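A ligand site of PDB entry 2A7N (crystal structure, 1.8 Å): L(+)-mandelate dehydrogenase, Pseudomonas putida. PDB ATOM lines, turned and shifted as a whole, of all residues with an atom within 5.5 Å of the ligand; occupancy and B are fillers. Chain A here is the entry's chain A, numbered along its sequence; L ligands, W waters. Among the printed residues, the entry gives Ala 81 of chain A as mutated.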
ATOM      1  N   TYR A  26       7.069  23.913 -22.543  1.00  0.00           N
ATOM      2  CA  TYR A  26       6.500  23.108 -23.619  1.00  0.00           C
ATOM      3  C   TYR A  26       4.992  23.048 -23.434  1.00  0.00           C
ATOM      4  O   TYR A  26       4.226  23.136 -24.394  1.00  0.00           O
ATOM      5  CB  TYR A  26       7.061  21.682 -23.580  1.00  0.00           C
ATOM      6  CG  TYR A  26       6.209  20.683 -24.334  1.00  0.00           C
ATOM      7  CD1 TYR A  26       6.082  20.757 -25.728  1.00  0.00           C
ATOM      8  CD2 TYR A  26       5.504  19.686 -23.664  1.00  0.00           C
ATOM      9  CE1 TYR A  26       5.269  19.853 -26.426  1.00  0.00           C
ATOM     10  CE2 TYR A  26       4.695  18.774 -24.350  1.00  0.00           C
ATOM     11  CZ  TYR A  26       4.579  18.868 -25.725  1.00  0.00           C
ATOM     12  OH  TYR A  26       3.770  17.984 -26.409  1.00  0.00           O
ATOM     13  N   LEU A  27       4.569  22.890 -22.177  1.00  0.00           N
ATOM     14  CA  LEU A  27       3.157  22.788 -21.827  1.00  0.00           C
ATOM     15  C   LEU A  27       2.365  24.085 -21.924  1.00  0.00           C
ATOM     16  O   LEU A  27       1.341  24.145 -22.594  1.00  0.00           O
ATOM     17  CB  LEU A  27       3.031  22.231 -20.398  1.00  0.00           C
ATOM     18  CG  LEU A  27       1.690  22.368 -19.666  1.00  0.00           C
ATOM     19  CD1 LEU A  27       0.624  21.537 -20.362  1.00  0.00           C
ATOM     20  CD2 LEU A  27       1.858  21.934 -18.211  1.00  0.00           C
ATOM     21  N   ASN A  40      -7.634  33.762 -25.997  1.00  0.00           N
ATOM     22  CA  ASN A  40      -8.439  32.573 -25.684  1.00  0.00           C
ATOM     23  C   ASN A  40      -9.082  32.711 -24.301  1.00  0.00           C
ATOM     24  O   ASN A  40     -10.189  32.220 -24.080  1.00  0.00           O
ATOM     25  CB  ASN A  40      -7.574  31.313 -25.707  1.00  0.00           C
ATOM     26  CG  ASN A  40      -7.273  30.818 -27.126  1.00  0.00           C
ATOM     27  OD1 ASN A  40      -6.559  29.827 -27.306  1.00  0.00           O
ATOM     28  ND2 ASN A  40      -7.821  31.495 -28.115  1.00  0.00           N
ATOM     29  N   GLY A  78      -9.055  16.166 -23.690  1.00  0.00           N
ATOM     30  CA  GLY A  78      -8.619  16.178 -25.073  1.00  0.00           C
ATOM     31  C   GLY A  78      -7.277  15.537 -25.351  1.00  0.00           C
ATOM     32  O   GLY A  78      -6.529  15.197 -24.423  1.00  0.00           O
ATOM     33  N   PRO A  79      -6.940  15.357 -26.627  1.00  0.00           N
ATOM     34  CA  PRO A  79      -5.669  14.747 -27.023  1.00  0.00           C
ATOM     35  C   PRO A  79      -4.469  15.683 -26.857  1.00  0.00           C
ATOM     36  O   PRO A  79      -4.457  16.788 -27.385  1.00  0.00           O
ATOM     37  CB  PRO A  79      -5.916  14.381 -28.481  1.00  0.00           C
ATOM     38  CG  PRO A  79      -6.786  15.510 -28.961  1.00  0.00           C
ATOM     39  CD  PRO A  79      -7.767  15.669 -27.812  1.00  0.00           C
ATOM     40  N   THR A  80      -3.479  15.233 -26.097  1.00  0.00           N
ATOM     41  CA  THR A  80      -2.267  16.010 -25.896  1.00  0.00           C
ATOM     42  C   THR A  80      -1.071  15.072 -25.985  1.00  0.00           C
ATOM     43  O   THR A  80      -1.084  13.978 -25.421  1.00  0.00           O
ATOM     44  CB  THR A  80      -2.267  16.763 -24.544  1.00  0.00           C
ATOM     45  OG1 THR A  80      -2.442  15.823 -23.473  1.00  0.00           O
ATOM     46  CG2 THR A  80      -3.389  17.797 -24.507  1.00  0.00           C
ATOM     47  N   ALA A  81      -0.050  15.490 -26.717  1.00  0.00           N
ATOM     48  CA  ALA A  81       1.146  14.689 -26.923  1.00  0.00           C
ATOM     49  C   ALA A  81       2.153  14.748 -25.786  1.00  0.00           C
ATOM     50  O   ALA A  81       2.219  15.724 -25.028  1.00  0.00           O
ATOM     51  CB  ALA A  81       1.824  15.111 -28.219  1.00  0.00           C
ATOM     52  N   SER A 108      -3.620  10.783 -28.045  1.00  0.00           N
ATOM     53  CA  SER A 108      -2.908  11.464 -29.122  1.00  0.00           C
ATOM     54  C   SER A 108      -2.099  10.480 -29.951  1.00  0.00           C
ATOM     55  O   SER A 108      -1.665   9.432 -29.462  1.00  0.00           O
ATOM     56  CB  SER A 108      -1.948  12.504 -28.533  1.00  0.00           C
ATOM     57  OG  SER A 108      -1.039  12.978 -29.521  1.00  0.00           O
ATOM     58  N   THR A 109      -1.902  10.813 -31.231  1.00  0.00           N
ATOM     59  CA  THR A 109      -1.109   9.967 -32.108  1.00  0.00           C
ATOM     60  C   THR A 109       0.311   9.963 -31.561  1.00  0.00           C
ATOM     61  O   THR A 109       1.038   8.981 -31.675  1.00  0.00           O
ATOM     62  CB  THR A 109      -1.105  10.526 -33.544  1.00  0.00           C
ATOM     63  OG1 THR A 109      -2.344  10.237 -34.184  1.00  0.00           O
ATOM     64  CG2 THR A 109       0.047   9.927 -34.352  1.00  0.00           C
ATOM     65  N   ALA A 110       0.698  11.090 -30.952  1.00  0.00           N
ATOM     66  CA  ALA A 110       2.025  11.263 -30.385  1.00  0.00           C
ATOM     67  C   ALA A 110       2.062  10.983 -28.879  1.00  0.00           C
ATOM     68  O   ALA A 110       2.779  11.656 -28.129  1.00  0.00           O
ATOM     69  CB  ALA A 110       2.537  12.664 -30.664  1.00  0.00           C
ATOM     70  N   GLN A 129      -7.113  10.274 -31.468  1.00  0.00           N
ATOM     71  CA  GLN A 129      -6.861  11.462 -32.261  1.00  0.00           C
ATOM     72  C   GLN A 129      -5.776  11.121 -33.267  1.00  0.00           C
ATOM     73  O   GLN A 129      -4.683  10.672 -32.896  1.00  0.00           O
ATOM     74  CB  GLN A 129      -6.416  12.623 -31.367  1.00  0.00           C
ATOM     75  CG  GLN A 129      -5.960  13.850 -32.139  1.00  0.00           C
ATOM     76  CD  GLN A 129      -4.491  13.798 -32.526  1.00  0.00           C
ATOM     77  OE1 GLN A 129      -4.114  14.104 -33.664  1.00  0.00           O
ATOM     78  NE2 GLN A 129      -3.634  13.420 -31.577  1.00  0.00           N
ATOM     79  N   TYR A 131      -3.131  12.010 -36.466  1.00  0.00           N
ATOM     80  CA  TYR A 131      -2.281  12.959 -37.177  1.00  0.00           C
ATOM     81  C   TYR A 131      -1.822  12.112 -38.359  1.00  0.00           C
ATOM     82  O   TYR A 131      -1.450  10.952 -38.171  1.00  0.00           O
ATOM     83  CB  TYR A 131      -1.047  13.355 -36.361  1.00  0.00           C
ATOM     84  CG  TYR A 131      -1.234  14.532 -35.428  1.00  0.00           C
ATOM     85  CD1 TYR A 131      -1.879  15.697 -35.851  1.00  0.00           C
ATOM     86  CD2 TYR A 131      -0.700  14.505 -34.140  1.00  0.00           C
ATOM     87  CE1 TYR A 131      -1.976  16.802 -35.006  1.00  0.00           C
ATOM     88  CE2 TYR A 131      -0.797  15.596 -33.295  1.00  0.00           C
ATOM     89  CZ  TYR A 131      -1.433  16.749 -33.731  1.00  0.00           C
ATOM     90  OH  TYR A 131      -1.517  17.834 -32.903  1.00  0.00           O
ATOM     91  N   THR A 156      -7.138  15.624 -36.502  1.00  0.00           N
ATOM     92  CA  THR A 156      -6.669  16.980 -36.202  1.00  0.00           C
ATOM     93  C   THR A 156      -6.085  17.551 -37.481  1.00  0.00           C
ATOM     94  O   THR A 156      -5.142  17.007 -38.053  1.00  0.00           O
ATOM     95  CB  THR A 156      -5.604  16.957 -35.097  1.00  0.00           C
ATOM     96  OG1 THR A 156      -6.199  16.450 -33.895  1.00  0.00           O
ATOM     97  CG2 THR A 156      -5.075  18.359 -34.835  1.00  0.00           C
ATOM     98  N   LYS A 231     -11.201  17.962 -35.986  1.00  0.00           N
ATOM     99  CA  LYS A 231     -10.739  18.932 -35.002  1.00  0.00           C
ATOM    100  C   LYS A 231      -9.821  20.000 -35.596  1.00  0.00           C
ATOM    101  O   LYS A 231      -9.047  19.718 -36.512  1.00  0.00           O
ATOM    102  CB  LYS A 231     -10.020  18.173 -33.882  1.00  0.00           C
ATOM    103  CG  LYS A 231      -9.340  19.012 -32.796  1.00  0.00           C
ATOM    104  CD  LYS A 231      -8.865  18.090 -31.656  1.00  0.00           C
ATOM    105  CE  LYS A 231      -8.165  18.841 -30.525  1.00  0.00           C
ATOM    106  NZ  LYS A 231      -6.745  19.166 -30.834  1.00  0.00           N
ATOM    107  N   SER A 253     -11.510  24.682 -32.711  1.00  0.00           N
ATOM    108  CA  SER A 253     -10.317  24.800 -31.884  1.00  0.00           C
ATOM    109  C   SER A 253      -9.164  25.526 -32.577  1.00  0.00           C
ATOM    110  O   SER A 253      -9.065  25.486 -33.799  1.00  0.00           O
ATOM    111  CB  SER A 253      -9.848  23.378 -31.519  1.00  0.00           C
ATOM    112  OG  SER A 253      -8.524  23.350 -31.015  1.00  0.00           O
ATOM    113  N   HIS A 255      -6.096  24.991 -31.284  1.00  0.00           N
ATOM    114  CA  HIS A 255      -5.015  24.221 -30.700  1.00  0.00           C
ATOM    115  C   HIS A 255      -4.417  24.871 -29.449  1.00  0.00           C
ATOM    116  O   HIS A 255      -3.210  24.846 -29.246  1.00  0.00           O
ATOM    117  CB  HIS A 255      -3.917  24.026 -31.759  1.00  0.00           C
ATOM    118  CG  HIS A 255      -3.173  22.729 -31.665  1.00  0.00           C
ATOM    119  ND1 HIS A 255      -3.420  21.669 -32.509  1.00  0.00           N
ATOM    120  CD2 HIS A 255      -2.183  22.324 -30.837  1.00  0.00           C
ATOM    121  CE1 HIS A 255      -2.610  20.668 -32.215  1.00  0.00           C
ATOM    122  NE2 HIS A 255      -1.847  21.037 -31.196  1.00  0.00           N
ATOM    123  N   GLY A 256      -5.268  25.465 -28.618  1.00  0.00           N
ATOM    124  CA  GLY A 256      -4.782  26.104 -27.403  1.00  0.00           C
ATOM    125  C   GLY A 256      -3.800  27.231 -27.669  1.00  0.00           C
ATOM    126  O   GLY A 256      -2.890  27.454 -26.879  1.00  0.00           O
ATOM    127  N   ARG A 258      -1.464  27.385 -29.771  1.00  0.00           N
ATOM    128  CA  ARG A 258      -0.114  26.884 -30.032  1.00  0.00           C
ATOM    129  C   ARG A 258       0.310  26.832 -31.502  1.00  0.00           C
ATOM    130  O   ARG A 258       1.473  26.528 -31.799  1.00  0.00           O
ATOM    131  CB  ARG A 258       0.034  25.494 -29.406  1.00  0.00           C
ATOM    132  CG  ARG A 258      -0.148  25.484 -27.892  1.00  0.00           C
ATOM    133  CD  ARG A 258      -0.448  24.084 -27.380  1.00  0.00           C
ATOM    134  NE  ARG A 258       0.664  23.143 -27.509  1.00  0.00           N
ATOM    135  CZ  ARG A 258       1.729  23.114 -26.695  1.00  0.00           C
ATOM    136  NH1 ARG A 258       1.842  23.979 -25.699  1.00  0.00           N
ATOM    137  NH2 ARG A 258       2.670  22.199 -26.878  1.00  0.00           N
ATOM    138  N   ASP A 284     -12.783  23.541 -27.770  1.00  0.00           N
ATOM    139  CA  ASP A 284     -11.727  23.625 -26.773  1.00  0.00           C
ATOM    140  C   ASP A 284     -10.947  24.910 -27.045  1.00  0.00           C
ATOM    141  O   ASP A 284     -11.273  25.646 -27.988  1.00  0.00           O
ATOM    142  CB  ASP A 284     -10.782  22.415 -26.811  1.00  0.00           C
ATOM    143  CG  ASP A 284      -9.881  22.384 -28.042  1.00  0.00           C
ATOM    144  OD1 ASP A 284      -9.637  23.437 -28.660  1.00  0.00           O
ATOM    145  OD2 ASP A 284      -9.389  21.278 -28.372  1.00  0.00           O
ATOM    146  N   SER A 285      -9.942  25.171 -26.212  1.00  0.00           N
ATOM    147  CA  SER A 285      -9.051  26.328 -26.313  1.00  0.00           C
ATOM    148  C   SER A 285      -9.398  27.485 -25.374  1.00  0.00           C
ATOM    149  O   SER A 285     -10.296  28.280 -25.656  1.00  0.00           O
ATOM    150  CB  SER A 285      -8.978  26.850 -27.742  1.00  0.00           C
ATOM    151  OG  SER A 285      -8.506  25.837 -28.617  1.00  0.00           O
ATOM    152  N   GLY A 286      -8.677  27.548 -24.248  1.00  0.00           N
ATOM    153  CA  GLY A 286      -8.884  28.609 -23.285  1.00  0.00           C
ATOM    154  C   GLY A 286      -9.766  28.310 -22.089  1.00  0.00           C
ATOM    155  O   GLY A 286      -9.898  29.135 -21.192  1.00  0.00           O
ATOM    156  N   PHE A 287     -10.380  27.120 -22.049  1.00  0.00           N
ATOM    157  CA  PHE A 287     -11.254  26.791 -20.931  1.00  0.00           C
ATOM    158  C   PHE A 287     -10.502  26.493 -19.634  1.00  0.00           C
ATOM    159  O   PHE A 287      -9.657  25.603 -19.584  1.00  0.00           O
ATOM    160  CB  PHE A 287     -12.162  25.621 -21.307  1.00  0.00           C
ATOM    161  CG  PHE A 287     -13.094  25.924 -22.458  1.00  0.00           C
ATOM    162  CD1 PHE A 287     -12.647  25.859 -23.765  1.00  0.00           C
ATOM    163  CD2 PHE A 287     -14.412  26.326 -22.214  1.00  0.00           C
ATOM    164  CE1 PHE A 287     -13.485  26.197 -24.838  1.00  0.00           C
ATOM    165  CE2 PHE A 287     -15.263  26.670 -23.270  1.00  0.00           C
ATOM    166  CZ  PHE A 287     -14.787  26.598 -24.582  1.00  0.00           C
ATOM    167  N   ARG A 288     -10.819  27.258 -18.590  1.00  0.00           N
ATOM    168  CA  ARG A 288     -10.181  27.102 -17.283  1.00  0.00           C
ATOM    169  C   ARG A 288     -11.193  27.111 -16.123  1.00  0.00           C
ATOM    170  O   ARG A 288     -10.989  26.422 -15.120  1.00  0.00           O
ATOM    171  CB  ARG A 288      -9.162  28.219 -17.066  1.00  0.00           C
ATOM    172  CG  ARG A 288      -8.065  28.301 -18.133  1.00  0.00           C
ATOM    173  CD  ARG A 288      -7.070  27.137 -18.037  1.00  0.00           C
ATOM    174  NE  ARG A 288      -5.982  27.290 -19.005  1.00  0.00           N
ATOM    175  CZ  ARG A 288      -6.089  27.023 -20.308  1.00  0.00           C
ATOM    176  NH1 ARG A 288      -7.236  26.574 -20.805  1.00  0.00           N
ATOM    177  NH2 ARG A 288      -5.063  27.227 -21.114  1.00  0.00           N
ATOM    178  N   LEU A 305     -13.683  20.156 -24.569  1.00  0.00           N
ATOM    179  CA  LEU A 305     -12.530  19.305 -24.324  1.00  0.00           C
ATOM    180  C   LEU A 305     -11.494  20.117 -23.545  1.00  0.00           C
ATOM    181  O   LEU A 305     -11.245  21.280 -23.852  1.00  0.00           O
ATOM    182  CB  LEU A 305     -11.888  18.820 -25.623  1.00  0.00           C
ATOM    183  CG  LEU A 305     -12.709  17.898 -26.537  1.00  0.00           C
ATOM    184  CD1 LEU A 305     -13.556  18.751 -27.490  1.00  0.00           C
ATOM    185  CD2 LEU A 305     -11.762  16.995 -27.340  1.00  0.00           C
ATOM    186  N   LEU A 306     -10.922  19.480 -22.534  1.00  0.00           N
ATOM    187  CA  LEU A 306      -9.907  20.104 -21.712  1.00  0.00           C
ATOM    188  C   LEU A 306      -8.523  19.765 -22.226  1.00  0.00           C
ATOM    189  O   LEU A 306      -8.241  18.623 -22.616  1.00  0.00           O
ATOM    190  CB  LEU A 306     -10.021  19.623 -20.259  1.00  0.00           C
ATOM    191  CG  LEU A 306     -11.355  19.897 -19.557  1.00  0.00           C
ATOM    192  CD1 LEU A 306     -11.288  19.416 -18.122  1.00  0.00           C
ATOM    193  CD2 LEU A 306     -11.656  21.387 -19.627  1.00  0.00           C
ATOM    194  N   GLY A 307      -7.659  20.768 -22.259  1.00  0.00           N
ATOM    195  CA  GLY A 307      -6.302  20.566 -22.712  1.00  0.00           C
ATOM    196  C   GLY A 307      -5.383  20.757 -21.518  1.00  0.00           C
ATOM    197  O   GLY A 307      -5.148  19.823 -20.752  1.00  0.00           O
ATOM    198  N   ARG A 308      -4.896  21.974 -21.348  1.00  0.00           N
ATOM    199  CA  ARG A 308      -3.987  22.271 -20.245  1.00  0.00           C
ATOM    200  C   ARG A 308      -4.581  22.131 -18.835  1.00  0.00           C
ATOM    201  O   ARG A 308      -3.862  21.769 -17.904  1.00  0.00           O
ATOM    202  CB  ARG A 308      -3.417  23.691 -20.403  1.00  0.00           C
ATOM    203  CG  ARG A 308      -2.522  23.900 -21.622  1.00  0.00           C
ATOM    204  CD  ARG A 308      -1.844  25.257 -21.535  1.00  0.00           C
ATOM    205  NE  ARG A 308      -1.095  25.663 -22.730  1.00  0.00           N
ATOM    206  CZ  ARG A 308      -1.642  26.102 -23.854  1.00  0.00           C
ATOM    207  NH1 ARG A 308      -2.963  26.199 -23.970  1.00  0.00           N
ATOM    208  NH2 ARG A 308      -0.872  26.508 -24.850  1.00  0.00           N
ATOM    209  N   ALA A 309      -5.879  22.412 -18.675  1.00  0.00           N
ATOM    210  CA  ALA A 309      -6.508  22.335 -17.360  1.00  0.00           C
ATOM    211  C   ALA A 309      -6.210  21.022 -16.644  1.00  0.00           C
ATOM    212  O   ALA A 309      -5.689  21.023 -15.529  1.00  0.00           O
ATOM    213  CB  ALA A 309      -8.025  22.519 -17.482  1.00  0.00           C
ATOM    214  N   LEU A 311      -4.003  18.843 -17.565  1.00  0.00           N
ATOM    215  CA  LEU A 311      -2.569  18.557 -17.590  1.00  0.00           C
ATOM    216  C   LEU A 311      -1.876  19.173 -16.364  1.00  0.00           C
ATOM    217  O   LEU A 311      -0.866  18.655 -15.910  1.00  0.00           O
ATOM    218  CB  LEU A 311      -1.916  19.078 -18.880  1.00  0.00           C
ATOM    219  CG  LEU A 311      -2.297  18.322 -20.156  1.00  0.00           C
ATOM    220  CD1 LEU A 311      -1.459  18.840 -21.325  1.00  0.00           C
ATOM    221  CD2 LEU A 311      -2.056  16.830 -19.961  1.00  0.00           C
HETATM  222  N1  LIG L   1      -4.022  18.340 -30.146  1.00  0.00           N
HETATM  223  C1  LIG L   1      -4.122  17.180 -30.909  1.00  0.00           C
HETATM  224  O1  LIG L   1      -5.037  16.980 -31.610  1.00  0.00           O
HETATM  225  N2  LIG L   1      -3.037  16.198 -30.782  1.00  0.00           N
HETATM  226  C2  LIG L   1      -1.873  16.323 -29.950  1.00  0.00           C
HETATM  227  O2  LIG L   1      -0.993  15.465 -29.860  1.00  0.00           O
HETATM  228  C3  LIG L   1      -1.799  17.578 -29.129  1.00  0.00           C
HETATM  229  N3  LIG L   1      -0.784  17.799 -28.246  1.00  0.00           N
HETATM  230  C4  LIG L   1      -0.797  18.895 -27.378  1.00  0.00           C
HETATM  231  C5  LIG L   1       0.220  19.027 -26.346  1.00  0.00           C
HETATM  232  C6  LIG L   1       0.194  20.089 -25.319  1.00  0.00           C
HETATM  233  C7  LIG L   1       1.246  20.112 -24.258  1.00  0.00           C
HETATM  234  C8  LIG L   1      -0.957  21.115 -25.360  1.00  0.00           C
HETATM  235  C9  LIG L   1      -1.140  22.230 -24.356  1.00  0.00           C
HETATM  236  C10 LIG L   1      -1.933  20.997 -26.395  1.00  0.00           C
HETATM  237  C11 LIG L   1      -1.936  19.914 -27.419  1.00  0.00           C
HETATM  238  N4  LIG L   1      -2.972  19.668 -28.438  1.00  0.00           N
HETATM  239  C12 LIG L   1      -2.979  18.537 -29.315  1.00  0.00           C
HETATM  240  C13 LIG L   1      -4.123  20.595 -28.486  1.00  0.00           C
HETATM  241  C14 LIG L   1      -5.235  20.153 -27.530  1.00  0.00           C
HETATM  242  O3  LIG L   1      -5.948  19.075 -28.015  1.00  0.00           O
HETATM  243  C15 LIG L   1      -6.257  21.238 -27.245  1.00  0.00           C
HETATM  244  O4  LIG L   1      -6.757  21.753 -28.534  1.00  0.00           O
HETATM  245  C16 LIG L   1      -5.754  22.506 -26.543  1.00  0.00           C
HETATM  246  O5  LIG L   1      -4.875  22.266 -25.466  1.00  0.00           O
HETATM  247  C17 LIG L   1      -6.957  23.248 -26.029  1.00  0.00           C
HETATM  248  O6  LIG L   1      -6.602  24.449 -25.277  1.00  0.00           O
HETATM  249  P1  LIG L   1      -6.289  24.664 -23.786  1.00  0.00           P
HETATM  250  O7  LIG L   1      -6.405  26.128 -23.447  1.00  0.00           O
HETATM  251  O8  LIG L   1      -4.913  24.105 -23.568  1.00  0.00           O
HETATM  252  O9  LIG L   1      -7.352  23.838 -23.100  1.00  0.00           O
HETATM  253  O   HOH W   1       1.245  16.989 -22.777  1.00  0.00           O
HETATM  254  O   HOH W   2      -8.676  18.886 -27.048  1.00  0.00           O
HETATM  255  O   HOH W   3      -5.548  28.307 -25.009  1.00  0.00           O
HETATM  256  O   HOH W   4      -8.109  23.270 -20.462  1.00  0.00           O
HETATM  257  O   HOH W   5       0.186  19.019 -30.983  1.00  0.00           O
HETATM  258  O   HOH W   6      -9.846  23.874 -23.679  1.00  0.00           O
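The side-chain hydroxyl (OG) of Ser 108 is in hydrogen-bond range of an oxygen (O2) of the ligand (2.5 Å).
The backbone NH of Ala 81 sits at hydrogen-bond distance from a nitrogen (N3) of the ligand.
O7 of the ligand is in salt-bridge range of NH1 of Arg 288.
The side-chain hydroxyl (OG1) of Thr 156 is in hydrogen-bond range of an oxygen (O1) of the ligand (2.6 Å).
O8 of the ligand is in hydrogen-bond range of N of Arg 308 (3.1 Å).
O4 of the ligand is in hydrogen-bond range of OD2 of Asp 284 (2.7 Å).
NH1 of Arg 308 lies within salt-bridge range of O8 of the ligand (2.9 Å).
The backbone NH of Gly 307 lies within hydrogen-bond range of an oxygen (O9) of the ligand.
The side-chain hydroxyl (OG) of Ser 253 is in hydrogen-bond range of an oxygen (O4) of the ligand (3.4 Å).
A nitrogen (N2) of the ligand sits close to the side-chain amide nitrogen of Gln 129, at 3.0 Å.
The side-chain hydroxyl of Tyr 131 sits at hydrogen-bond distance from a nitrogen (N2) of the ligand, 3.1 Å away.
O1 of the ligand lies within hydrogen-bond range of NZ of Lys 231 (2.9 Å).
An oxygen (O3) of the ligand sits at hydrogen-bond distance from the backbone carbonyl oxygen (O) of Pro 79, at 2.8 Å.
N of Gly 286 is in hydrogen-bond range of O7 of the ligand (2.8 Å).
O of Leu 27 sits at hydrogen-bond distance from NH1 of Arg 258 (3.1 Å).
The backbone NH (N) of His 255 is in hydrogen-bond range of the side-chain hydroxyl (OG) of Ser 253, at 2.9 Å.
OG of Ser 108 sits close to NE2 of Gln 129, 3.3 Å away.
The side-chain hydroxyl (OG) of Ser 285 lies within hydrogen-bond range of the side-chain hydroxyl (OG) of Ser 253 (3.5 Å).
O of Gln 129 is in hydrogen-bond range of OG1 of Thr 109.
The guanidinium group (NH2) of Arg 308 is in hydrogen-bond range of the backbone carbonyl oxygen (O) of Gly 256 (3.0 Å).
The backbone NH of Ala 110 lies within hydrogen-bond range of the side-chain hydroxyl of Ser 108.
The side-chain carboxylate of Asp 284 is in hydrogen-bond range of the side-chain hydroxyl of Ser 253, at 2.6 Å.
A ring nitrogen (NE2) of His 255 lies close to a nitrogen (N4) of the ligand, at 3.3 Å.
Tyr 26 touches the ligand.
O of Leu 27 touches C9 of the ligand, at 3.6 Å.
Thr 80 touches the ligand.
Gly 256 touches the ligand (CA to O6, 3.3 Å).
Arg 258 touches the ligand.
Ser 285 touches the ligand.
Hydrophobic or aromatic side chains that line the ligand: Tyr 26, Pro 79, Ala 81, Tyr 131 and His 255.
20 residues have an atom within 4 Å of the ligand: Tyr 26, Leu 27, Pro 79, Thr 80, Ala 81, Ser 108, Gln 129, Tyr 131, Thr 156, Lys 231, Ser 253, His 255, Gly 256, Arg 258, Asp 284, Ser 285, Gly 286, Arg 288, Gly 307 and Arg 308.
Along chain A the residues within 4 Å of the ligand span positions 26 to 308.
Water W6 lies within hydrogen-bond range of O9 of the ligand (2.6 Å), N of Ser 285 (2.8 Å) and O of Leu 305 (3.0 Å).
Water W3 lies within hydrogen-bond range of O7 of the ligand (2.8 Å), OD1 of Asn 40 (2.9 Å), N of Gly 286 (3.3 Å), O of Gly 256 (3.4 Å) and NH1 of Arg 308 (3.5 Å).
Water W2 lies within hydrogen-bond range of OD2 of Asp 284 and O3 of the ligand.
Water W5 lies within hydrogen-bond range of OH of Tyr 131 (2.8 Å), NE2 of His 255 (2.9 Å) and N3 of the ligand (3.1 Å).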
